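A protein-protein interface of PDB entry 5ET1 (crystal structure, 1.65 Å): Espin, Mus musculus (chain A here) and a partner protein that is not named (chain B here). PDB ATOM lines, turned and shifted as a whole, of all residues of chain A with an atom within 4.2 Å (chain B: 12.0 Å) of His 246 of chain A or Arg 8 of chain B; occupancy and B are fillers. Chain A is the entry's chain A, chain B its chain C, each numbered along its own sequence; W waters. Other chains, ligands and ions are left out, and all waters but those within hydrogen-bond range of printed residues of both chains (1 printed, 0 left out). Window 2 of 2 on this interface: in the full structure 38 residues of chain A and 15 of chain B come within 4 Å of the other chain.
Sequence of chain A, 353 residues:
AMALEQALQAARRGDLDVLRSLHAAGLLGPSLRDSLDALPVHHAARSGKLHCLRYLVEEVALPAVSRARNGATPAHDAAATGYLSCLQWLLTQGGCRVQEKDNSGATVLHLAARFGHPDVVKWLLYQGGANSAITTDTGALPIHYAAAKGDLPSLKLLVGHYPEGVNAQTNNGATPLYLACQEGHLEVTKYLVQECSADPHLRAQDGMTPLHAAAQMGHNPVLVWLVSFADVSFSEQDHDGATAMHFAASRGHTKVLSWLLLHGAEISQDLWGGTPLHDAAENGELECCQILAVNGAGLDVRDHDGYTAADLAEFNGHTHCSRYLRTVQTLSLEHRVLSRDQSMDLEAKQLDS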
ATOM      1  N   ASP A 240      20.507 -24.809  11.194  1.00  0.00           N
ATOM      2  CA  ASP A 240      19.737 -23.748  11.830  1.00  0.00           C
ATOM      3  C   ASP A 240      18.234 -23.893  11.620  1.00  0.00           C
ATOM      4  O   ASP A 240      17.483 -23.007  12.035  1.00  0.00           O
ATOM      5  CB  ASP A 240      20.181 -22.373  11.309  1.00  0.00           C
ATOM      6  CG  ASP A 240      21.548 -21.975  11.812  1.00  0.00           C
ATOM      7  OD1 ASP A 240      21.857 -22.263  12.985  1.00  0.00           O
ATOM      8  OD2 ASP A 240      22.318 -21.383  11.027  1.00  0.00           O
ATOM      9  N   ALA A 242      16.903 -23.860   8.589  1.00  0.00           N
ATOM     10  CA  ALA A 242      16.562 -23.124   7.380  1.00  0.00           C
ATOM     11  C   ALA A 242      16.234 -24.069   6.233  1.00  0.00           C
ATOM     12  O   ALA A 242      16.920 -25.075   6.022  1.00  0.00           O
ATOM     13  CB  ALA A 242      17.719 -22.216   6.970  1.00  0.00           C
ATOM     14  N   THR A 243      15.190 -23.729   5.480  1.00  0.00           N
ATOM     15  CA  THR A 243      14.833 -24.413   4.246  1.00  0.00           C
ATOM     16  C   THR A 243      15.381 -23.653   3.042  1.00  0.00           C
ATOM     17  O   THR A 243      15.842 -22.517   3.149  1.00  0.00           O
ATOM     18  CB  THR A 243      13.313 -24.537   4.111  1.00  0.00           C
ATOM     19  OG1 THR A 243      12.754 -23.228   3.916  1.00  0.00           O
ATOM     20  CG2 THR A 243      12.703 -25.160   5.377  1.00  0.00           C
ATOM     21  N   ALA A 244      15.285 -24.283   1.869  1.00  0.00           N
ATOM     22  CA  ALA A 244      15.624 -23.584   0.631  1.00  0.00           C
ATOM     23  C   ALA A 244      14.911 -22.242   0.540  1.00  0.00           C
ATOM     24  O   ALA A 244      15.473 -21.261   0.044  1.00  0.00           O
ATOM     25  CB  ALA A 244      15.250 -24.437  -0.580  1.00  0.00           C
ATOM     26  N   MET A 245      13.668 -22.185   1.005  1.00  0.00           N
ATOM     27  CA  MET A 245      12.896 -20.960   0.848  1.00  0.00           C
ATOM     28  C   MET A 245      13.500 -19.820   1.666  1.00  0.00           C
ATOM     29  O   MET A 245      13.517 -18.672   1.211  1.00  0.00           O
ATOM     30  CB  MET A 245      11.441 -21.207   1.238  1.00  0.00           C
ATOM     31  CG  MET A 245      10.485 -20.153   0.711  1.00  0.00           C
ATOM     32  SD  MET A 245       8.783 -20.328   1.272  1.00  0.00           S
ATOM     33  CE  MET A 245       8.295 -21.848   0.447  1.00  0.00           C
ATOM     34  N   HIS A 246      13.990 -20.119   2.875  1.00  0.00           N
ATOM     35  CA  HIS A 246      14.684 -19.110   3.674  1.00  0.00           C
ATOM     36  C   HIS A 246      15.849 -18.504   2.899  1.00  0.00           C
ATOM     37  O   HIS A 246      16.004 -17.278   2.831  1.00  0.00           O
ATOM     38  CB  HIS A 246      15.209 -19.721   4.977  1.00  0.00           C
ATOM     39  CG  HIS A 246      14.157 -20.039   5.992  1.00  0.00           C
ATOM     40  ND1 HIS A 246      13.530 -21.266   6.050  1.00  0.00           N
ATOM     41  CD2 HIS A 246      13.646 -19.306   7.013  1.00  0.00           C
ATOM     42  CE1 HIS A 246      12.672 -21.272   7.056  1.00  0.00           C
ATOM     43  NE2 HIS A 246      12.720 -20.094   7.653  1.00  0.00           N
ATOM     44  N   PHE A 247      16.698 -19.358   2.324  1.00  0.00           N
ATOM     45  CA  PHE A 247      17.875 -18.863   1.623  1.00  0.00           C
ATOM     46  C   PHE A 247      17.496 -18.001   0.425  1.00  0.00           C
ATOM     47  O   PHE A 247      18.089 -16.937   0.208  1.00  0.00           O
ATOM     48  CB  PHE A 247      18.759 -20.038   1.200  1.00  0.00           C
ATOM     49  CG  PHE A 247      19.599 -20.574   2.322  1.00  0.00           C
ATOM     50  CD1 PHE A 247      20.728 -19.890   2.741  1.00  0.00           C
ATOM     51  CD2 PHE A 247      19.242 -21.742   2.977  1.00  0.00           C
ATOM     52  CE1 PHE A 247      21.503 -20.374   3.791  1.00  0.00           C
ATOM     53  CE2 PHE A 247      20.008 -22.225   4.029  1.00  0.00           C
ATOM     54  CZ  PHE A 247      21.129 -21.542   4.432  1.00  0.00           C
ATOM     55  N   ALA A 248      16.517 -18.448  -0.370  1.00  0.00           N
ATOM     56  CA  ALA A 248      16.107 -17.683  -1.544  1.00  0.00           C
ATOM     57  C   ALA A 248      15.534 -16.333  -1.144  1.00  0.00           C
ATOM     58  O   ALA A 248      15.870 -15.302  -1.741  1.00  0.00           O
ATOM     59  CB  ALA A 248      15.078 -18.474  -2.351  1.00  0.00           C
ATOM     60  N   ALA A 249      14.669 -16.320  -0.124  1.00  0.00           N
ATOM     61  CA  ALA A 249      14.064 -15.066   0.320  1.00  0.00           C
ATOM     62  C   ALA A 249      15.112 -14.102   0.867  1.00  0.00           C
ATOM     63  O   ALA A 249      15.020 -12.885   0.655  1.00  0.00           O
ATOM     64  CB  ALA A 249      13.000 -15.348   1.383  1.00  0.00           C
ATOM     65  N   SER A 250      16.118 -14.624   1.571  1.00  0.00           N
ATOM     66  CA  SER A 250      17.130 -13.758   2.173  1.00  0.00           C
ATOM     67  C   SER A 250      17.962 -13.035   1.121  1.00  0.00           C
ATOM     68  O   SER A 250      18.499 -11.953   1.390  1.00  0.00           O
ATOM     69  CB  SER A 250      18.049 -14.570   3.092  1.00  0.00           C
ATOM     70  OG  SER A 250      19.046 -15.257   2.343  1.00  0.00           O
ATOM     71  N   SER A 268       7.901 -22.087   6.746  1.00  0.00           N
ATOM     72  CA  SER A 268       8.154 -22.644   8.066  1.00  0.00           C
ATOM     73  C   SER A 268       9.151 -21.786   8.835  1.00  0.00           C
ATOM     74  O   SER A 268       9.931 -21.028   8.251  1.00  0.00           O
ATOM     75  CB  SER A 268       8.685 -24.082   7.954  1.00  0.00           C
ATOM     76  OG  SER A 268       7.981 -24.801   6.956  1.00  0.00           O
ATOM     77  N   ASP A 270      12.495 -21.414  11.186  1.00  0.00           N
ATOM     78  CA  ASP A 270      13.737 -22.098  11.503  1.00  0.00           C
ATOM     79  C   ASP A 270      13.847 -22.251  13.018  1.00  0.00           C
ATOM     80  O   ASP A 270      12.930 -21.909  13.772  1.00  0.00           O
ATOM     81  CB  ASP A 270      14.936 -21.360  10.895  1.00  0.00           C
ATOM     82  CG  ASP A 270      15.127 -19.945  11.448  1.00  0.00           C
ATOM     83  OD1 ASP A 270      15.954 -19.203  10.868  1.00  0.00           O
ATOM     84  OD2 ASP A 270      14.482 -19.565  12.445  1.00  0.00           O
ATOM     85  N   GLY A 274      12.272 -17.786  12.793  1.00  0.00           N
ATOM     86  CA  GLY A 274      12.079 -16.938  11.629  1.00  0.00           C
ATOM     87  C   GLY A 274      11.555 -17.721  10.436  1.00  0.00           C
ATOM     88  O   GLY A 274      12.016 -18.821  10.147  1.00  0.00           O
ATOM     89  N   THR A 275      10.565 -17.146   9.763  1.00  0.00           N
ATOM     90  CA  THR A 275      10.073 -17.670   8.497  1.00  0.00           C
ATOM     91  C   THR A 275      10.858 -17.047   7.361  1.00  0.00           C
ATOM     92  O   THR A 275      11.642 -16.119   7.570  1.00  0.00           O
ATOM     93  CB  THR A 275       8.582 -17.364   8.347  1.00  0.00           C
ATOM     94  OG1 THR A 275       8.411 -15.988   7.976  1.00  0.00           O
ATOM     95  CG2 THR A 275       7.836 -17.647   9.652  1.00  0.00           C
ATOM     96  N   PRO A 276      10.685 -17.537   6.130  1.00  0.00           N
ATOM     97  CA  PRO A 276      11.308 -16.843   4.993  1.00  0.00           C
ATOM     98  C   PRO A 276      10.856 -15.400   4.858  1.00  0.00           C
ATOM     99  O   PRO A 276      11.587 -14.590   4.276  1.00  0.00           O
ATOM    100  CB  PRO A 276      10.875 -17.691   3.790  1.00  0.00           C
ATOM    101  CG  PRO A 276      10.724 -19.071   4.373  1.00  0.00           C
ATOM    102  CD  PRO A 276      10.079 -18.818   5.717  1.00  0.00           C
ATOM    103  N   ASP A 279      13.313 -13.427   6.763  1.00  0.00           N
ATOM    104  CA  ASP A 279      14.550 -13.288   5.996  1.00  0.00           C
ATOM    105  C   ASP A 279      14.430 -12.202   4.934  1.00  0.00           C
ATOM    106  O   ASP A 279      15.346 -11.387   4.753  1.00  0.00           O
ATOM    107  CB  ASP A 279      14.919 -14.611   5.320  1.00  0.00           C
ATOM    108  CG  ASP A 279      15.341 -15.685   6.303  1.00  0.00           C
ATOM    109  OD1 ASP A 279      14.466 -16.407   6.811  1.00  0.00           O
ATOM    110  OD2 ASP A 279      16.550 -15.830   6.544  1.00  0.00           O
ATOM    111  N   ARG B   7      22.129 -11.809   9.109  1.00  0.00           N
ATOM    112  CA  ARG B   7      22.560 -13.177   9.386  1.00  0.00           C
ATOM    113  C   ARG B   7      22.630 -14.020   8.123  1.00  0.00           C
ATOM    114  O   ARG B   7      23.691 -14.147   7.504  1.00  0.00           O
ATOM    115  CB  ARG B   7      21.617 -13.848  10.389  1.00  0.00           C
ATOM    116  N   ARG B   8      21.486 -14.595   7.746  1.00  0.00           N
ATOM    117  CA  ARG B   8      21.478 -15.605   6.693  1.00  0.00           C
ATOM    118  C   ARG B   8      21.990 -15.045   5.368  1.00  0.00           C
ATOM    119  O   ARG B   8      22.744 -15.719   4.655  1.00  0.00           O
ATOM    120  CB  ARG B   8      20.067 -16.183   6.536  1.00  0.00           C
ATOM    121  CG  ARG B   8      19.989 -17.353   5.583  1.00  0.00           C
ATOM    122  CD  ARG B   8      18.783 -18.244   5.877  1.00  0.00           C
ATOM    123  NE  ARG B   8      18.942 -18.976   7.128  1.00  0.00           N
ATOM    124  CZ  ARG B   8      18.108 -18.916   8.167  1.00  0.00           C
ATOM    125  NH1 ARG B   8      17.012 -18.165   8.129  1.00  0.00           N
ATOM    126  NH2 ARG B   8      18.373 -19.631   9.253  1.00  0.00           N
ATOM    127  N   ARG B   9      21.611 -13.808   5.025  1.00  0.00           N
ATOM    128  CA  ARG B   9      22.080 -13.228   3.767  1.00  0.00           C
ATOM    129  C   ARG B   9      23.597 -13.070   3.745  1.00  0.00           C
ATOM    130  O   ARG B   9      24.218 -13.201   2.685  1.00  0.00           O
ATOM    131  CB  ARG B   9      21.421 -11.873   3.516  1.00  0.00           C
ATOM    132  CG  ARG B   9      21.832 -11.223   2.197  1.00  0.00           C
ATOM    133  CD  ARG B   9      21.435  -9.760   2.162  1.00  0.00           C
ATOM    134  NE  ARG B   9      21.751  -9.108   0.891  1.00  0.00           N
ATOM    135  CZ  ARG B   9      20.864  -8.877  -0.075  1.00  0.00           C
ATOM    136  NH1 ARG B   9      19.598  -9.253   0.079  1.00  0.00           N
ATOM    137  NH2 ARG B   9      21.240  -8.265  -1.194  1.00  0.00           N
ATOM    138  N   CYS B  10      24.210 -12.789   4.897  1.00  0.00           N
ATOM    139  CA  CYS B  10      25.653 -12.597   4.964  1.00  0.00           C
ATOM    140  C   CYS B  10      26.436 -13.893   4.877  1.00  0.00           C
ATOM    141  O   CYS B  10      27.664 -13.845   4.731  1.00  0.00           O
ATOM    142  CB  CYS B  10      26.031 -11.876   6.257  1.00  0.00           C
ATOM    143  SG  CYS B  10      25.197 -10.307   6.459  1.00  0.00           S
ATOM    144  N   GLN B  11      25.778 -15.045   4.968  1.00  0.00           N
ATOM    145  CA  GLN B  11      26.501 -16.290   4.793  1.00  0.00           C
ATOM    146  C   GLN B  11      27.042 -16.354   3.374  1.00  0.00           C
ATOM    147  O   GLN B  11      26.302 -16.172   2.403  1.00  0.00           O
ATOM    148  CB  GLN B  11      25.607 -17.492   5.084  1.00  0.00           C
ATOM    149  CG  GLN B  11      26.407 -18.767   5.278  1.00  0.00           C
ATOM    150  CD  GLN B  11      25.555 -19.960   5.652  1.00  0.00           C
ATOM    151  OE1 GLN B  11      24.374 -19.822   5.976  1.00  0.00           O
ATOM    152  NE2 GLN B  11      26.154 -21.146   5.611  1.00  0.00           N
ATOM    153  N   GLN B  12      28.320 -16.575   3.259  1.00  0.00           N
ATOM    154  CA  GLN B  12      28.966 -16.591   1.962  1.00  0.00           C
ATOM    155  C   GLN B  12      28.890 -17.980   1.349  1.00  0.00           C
ATOM    156  O   GLN B  12      28.738 -18.981   2.060  1.00  0.00           O
ATOM    157  CB  GLN B  12      30.419 -16.154   2.101  1.00  0.00           C
ATOM    158  CG  GLN B  12      30.571 -14.717   2.611  1.00  0.00           C
ATOM    159  CD  GLN B  12      31.997 -14.205   2.485  1.00  0.00           C
ATOM    160  OE1 GLN B  12      32.948 -14.986   2.399  1.00  0.00           O
ATOM    161  NE2 GLN B  12      32.151 -12.887   2.460  1.00  0.00           N
ATOM    162  N   PRO B  13      28.980 -18.075   0.025  1.00  0.00           N
ATOM    163  CA  PRO B  13      29.068 -19.393  -0.607  1.00  0.00           C
ATOM    164  C   PRO B  13      30.328 -20.113  -0.152  1.00  0.00           C
ATOM    165  O   PRO B  13      31.287 -19.505   0.327  1.00  0.00           O
ATOM    166  CB  PRO B  13      29.118 -19.069  -2.106  1.00  0.00           C
ATOM    167  CG  PRO B  13      29.587 -17.629  -2.168  1.00  0.00           C
ATOM    168  CD  PRO B  13      28.981 -16.983  -0.966  1.00  0.00           C
ATOM    169  N   LYS B  14      30.314 -21.434  -0.299  1.00  0.00           N
ATOM    170  CA  LYS B  14      31.508 -22.211   0.006  1.00  0.00           C
ATOM    171  C   LYS B  14      32.575 -21.926  -1.037  1.00  0.00           C
ATOM    172  O   LYS B  14      32.335 -22.038  -2.245  1.00  0.00           O
ATOM    173  CB  LYS B  14      31.201 -23.706   0.048  1.00  0.00           C
ATOM    174  CG  LYS B  14      30.672 -24.204   1.378  1.00  0.00           C
ATOM    175  CD  LYS B  14      29.293 -23.680   1.639  1.00  0.00           C
ATOM    176  CE  LYS B  14      28.738 -24.180   2.963  1.00  0.00           C
ATOM    177  NZ  LYS B  14      27.314 -23.773   3.044  1.00  0.00           N
HETATM  178  O   HOH W   1      20.881 -20.966   8.226  1.00  0.00           O
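Of chain B, only Arg 8 (3.7 Å) comes within 4 Å of His 246 of chain A.
Of chain A, only Asp 240 (3.9 Å), Ala 242 (3.5 Å), His 246 (3.7 Å), Phe 247 (3.8 Å), Ser 250 (3.97 Å), Asp 270 (2.9 Å) and Asp 279 (2.9 Å) come within 4 Å of Arg 8 of chain B.
Asp 240 of chain A touches just one residue of chain B: Arg 8 (3.9 Å).
Ala 242 of chain A touches one residue of chain B.
No residue of chain B comes within 4 Å of Thr 243 of chain A.
No residue of chain B comes within 4 Å of Met 245 of chain A.
Of chain B, only Arg 8 (3.8 Å) and Gln 11 (3.6 Å) come within 4 Å of Phe 247 of chain A.
No residue of chain B comes within 4 Å of Ala 248 of chain A.
Ser 250 of chain A touches just these residues of chain B: Arg 8 and Arg 9.
Of chain B, only Arg 8 comes within 4 Å of Asp 270 of chain A.
No residue of chain B comes within 4 Å of Thr 275 of chain A.
No residue of chain B comes within 4 Å of Pro 276 of chain A.
Of chain B, only Arg 8 comes within 4 Å of Asp 279 of chain A.
Of the printed residues of chain A, Arg 9 of chain B touches Ser 250 (3.2 Å).
Of the printed residues of chain A, Gln 11 of chain B touches Phe 247.
Arg 7 of chain B touches none of the printed residues of chain A.
Pro 13 of chain B touches none of the printed residues of chain A.
The nearest printed residue of chain A that does not touch Arg 8 of chain B is Gly 274 of chain A (5.4 Å).
OD2 of Asp 279 of chain A is in salt-bridge range of NH1 of Arg 8 of chain B, at 2.9 Å.
The side-chain carboxylate (OD1) of Asp 270 of chain A is in salt-bridge range of the guanidinium group (NH2) of Arg 8 of chain B (2.9 Å).
The guanidinium group of Arg 9 of chain B sits at hydrogen-bond distance from the backbone carbonyl oxygen of Ser 250 of chain A (3.2 Å).
N of Gly 274 of chain A sits at hydrogen-bond distance from OD2 of Asp 270 of chain A, 2.9 Å away.
The side-chain hydroxyl (OG1) of Thr 243 of chain A is in hydrogen-bond range of a ring nitrogen (ND1) of His 246 of chain A (3.0 Å).
NE2 of His 246 of chain A lies within hydrogen-bond range of O of Gly 274 of chain A (2.9 Å).
OG of Ser 250 of chain A lies within hydrogen-bond range of O of Phe 247 of chain A, at 2.9 Å.
NE2 of His 246 of chain A lies close to O of Ser 268 of chain A (3.0 Å).
Water W1 bridges the guanidinium group (NE) of Arg 8 of chain B (3.0 Å) and the side-chain carboxylate (OD2) of Asp 240 of chain A (3.2 Å).
Of the 8 printed residues of chain B, 3 touch a printed residue of chain A.
Printed residues of chain B that touch a printed residue of chain A: Arg 8, Arg 9 and Gln 11.
Of the 16 printed residues of chain A, 7 touch a printed residue of chain B.
Printed residues of chain A that touch a printed residue of chain B: Asp 240, Ala 242, His 246, Phe 247, Ser 250, Asp 270 and Asp 279.
Hydrophobic or aromatic side chains of chain A that line the printed part of chain B: Ala 242, His 246 and Phe 247.
Among the printed residues, Asp or Glu carboxylates within 4 Å of a Lys or Arg side-chain nitrogen of the other chain: Asp 270 of chain A with Arg 8 of chain B and Asp 279 of chain A with Arg 8 of chain B.
Among the printed residues, merely in contact across the chains: Asp 240 of chain A with Arg 8 of chain B (3.9 Å), Ala 242 of chain A with Arg 8 of chain B (3.5 Å), His 246 of chain A with Arg 8 of chain B (3.7 Å), Phe 247 of chain A with Arg 8 of chain B (3.8 Å), Phe 247 of chain A with Gln 11 of chain B (3.6 Å) and Ser 250 of chain A with Arg 8 of chain B (3.97 Å).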
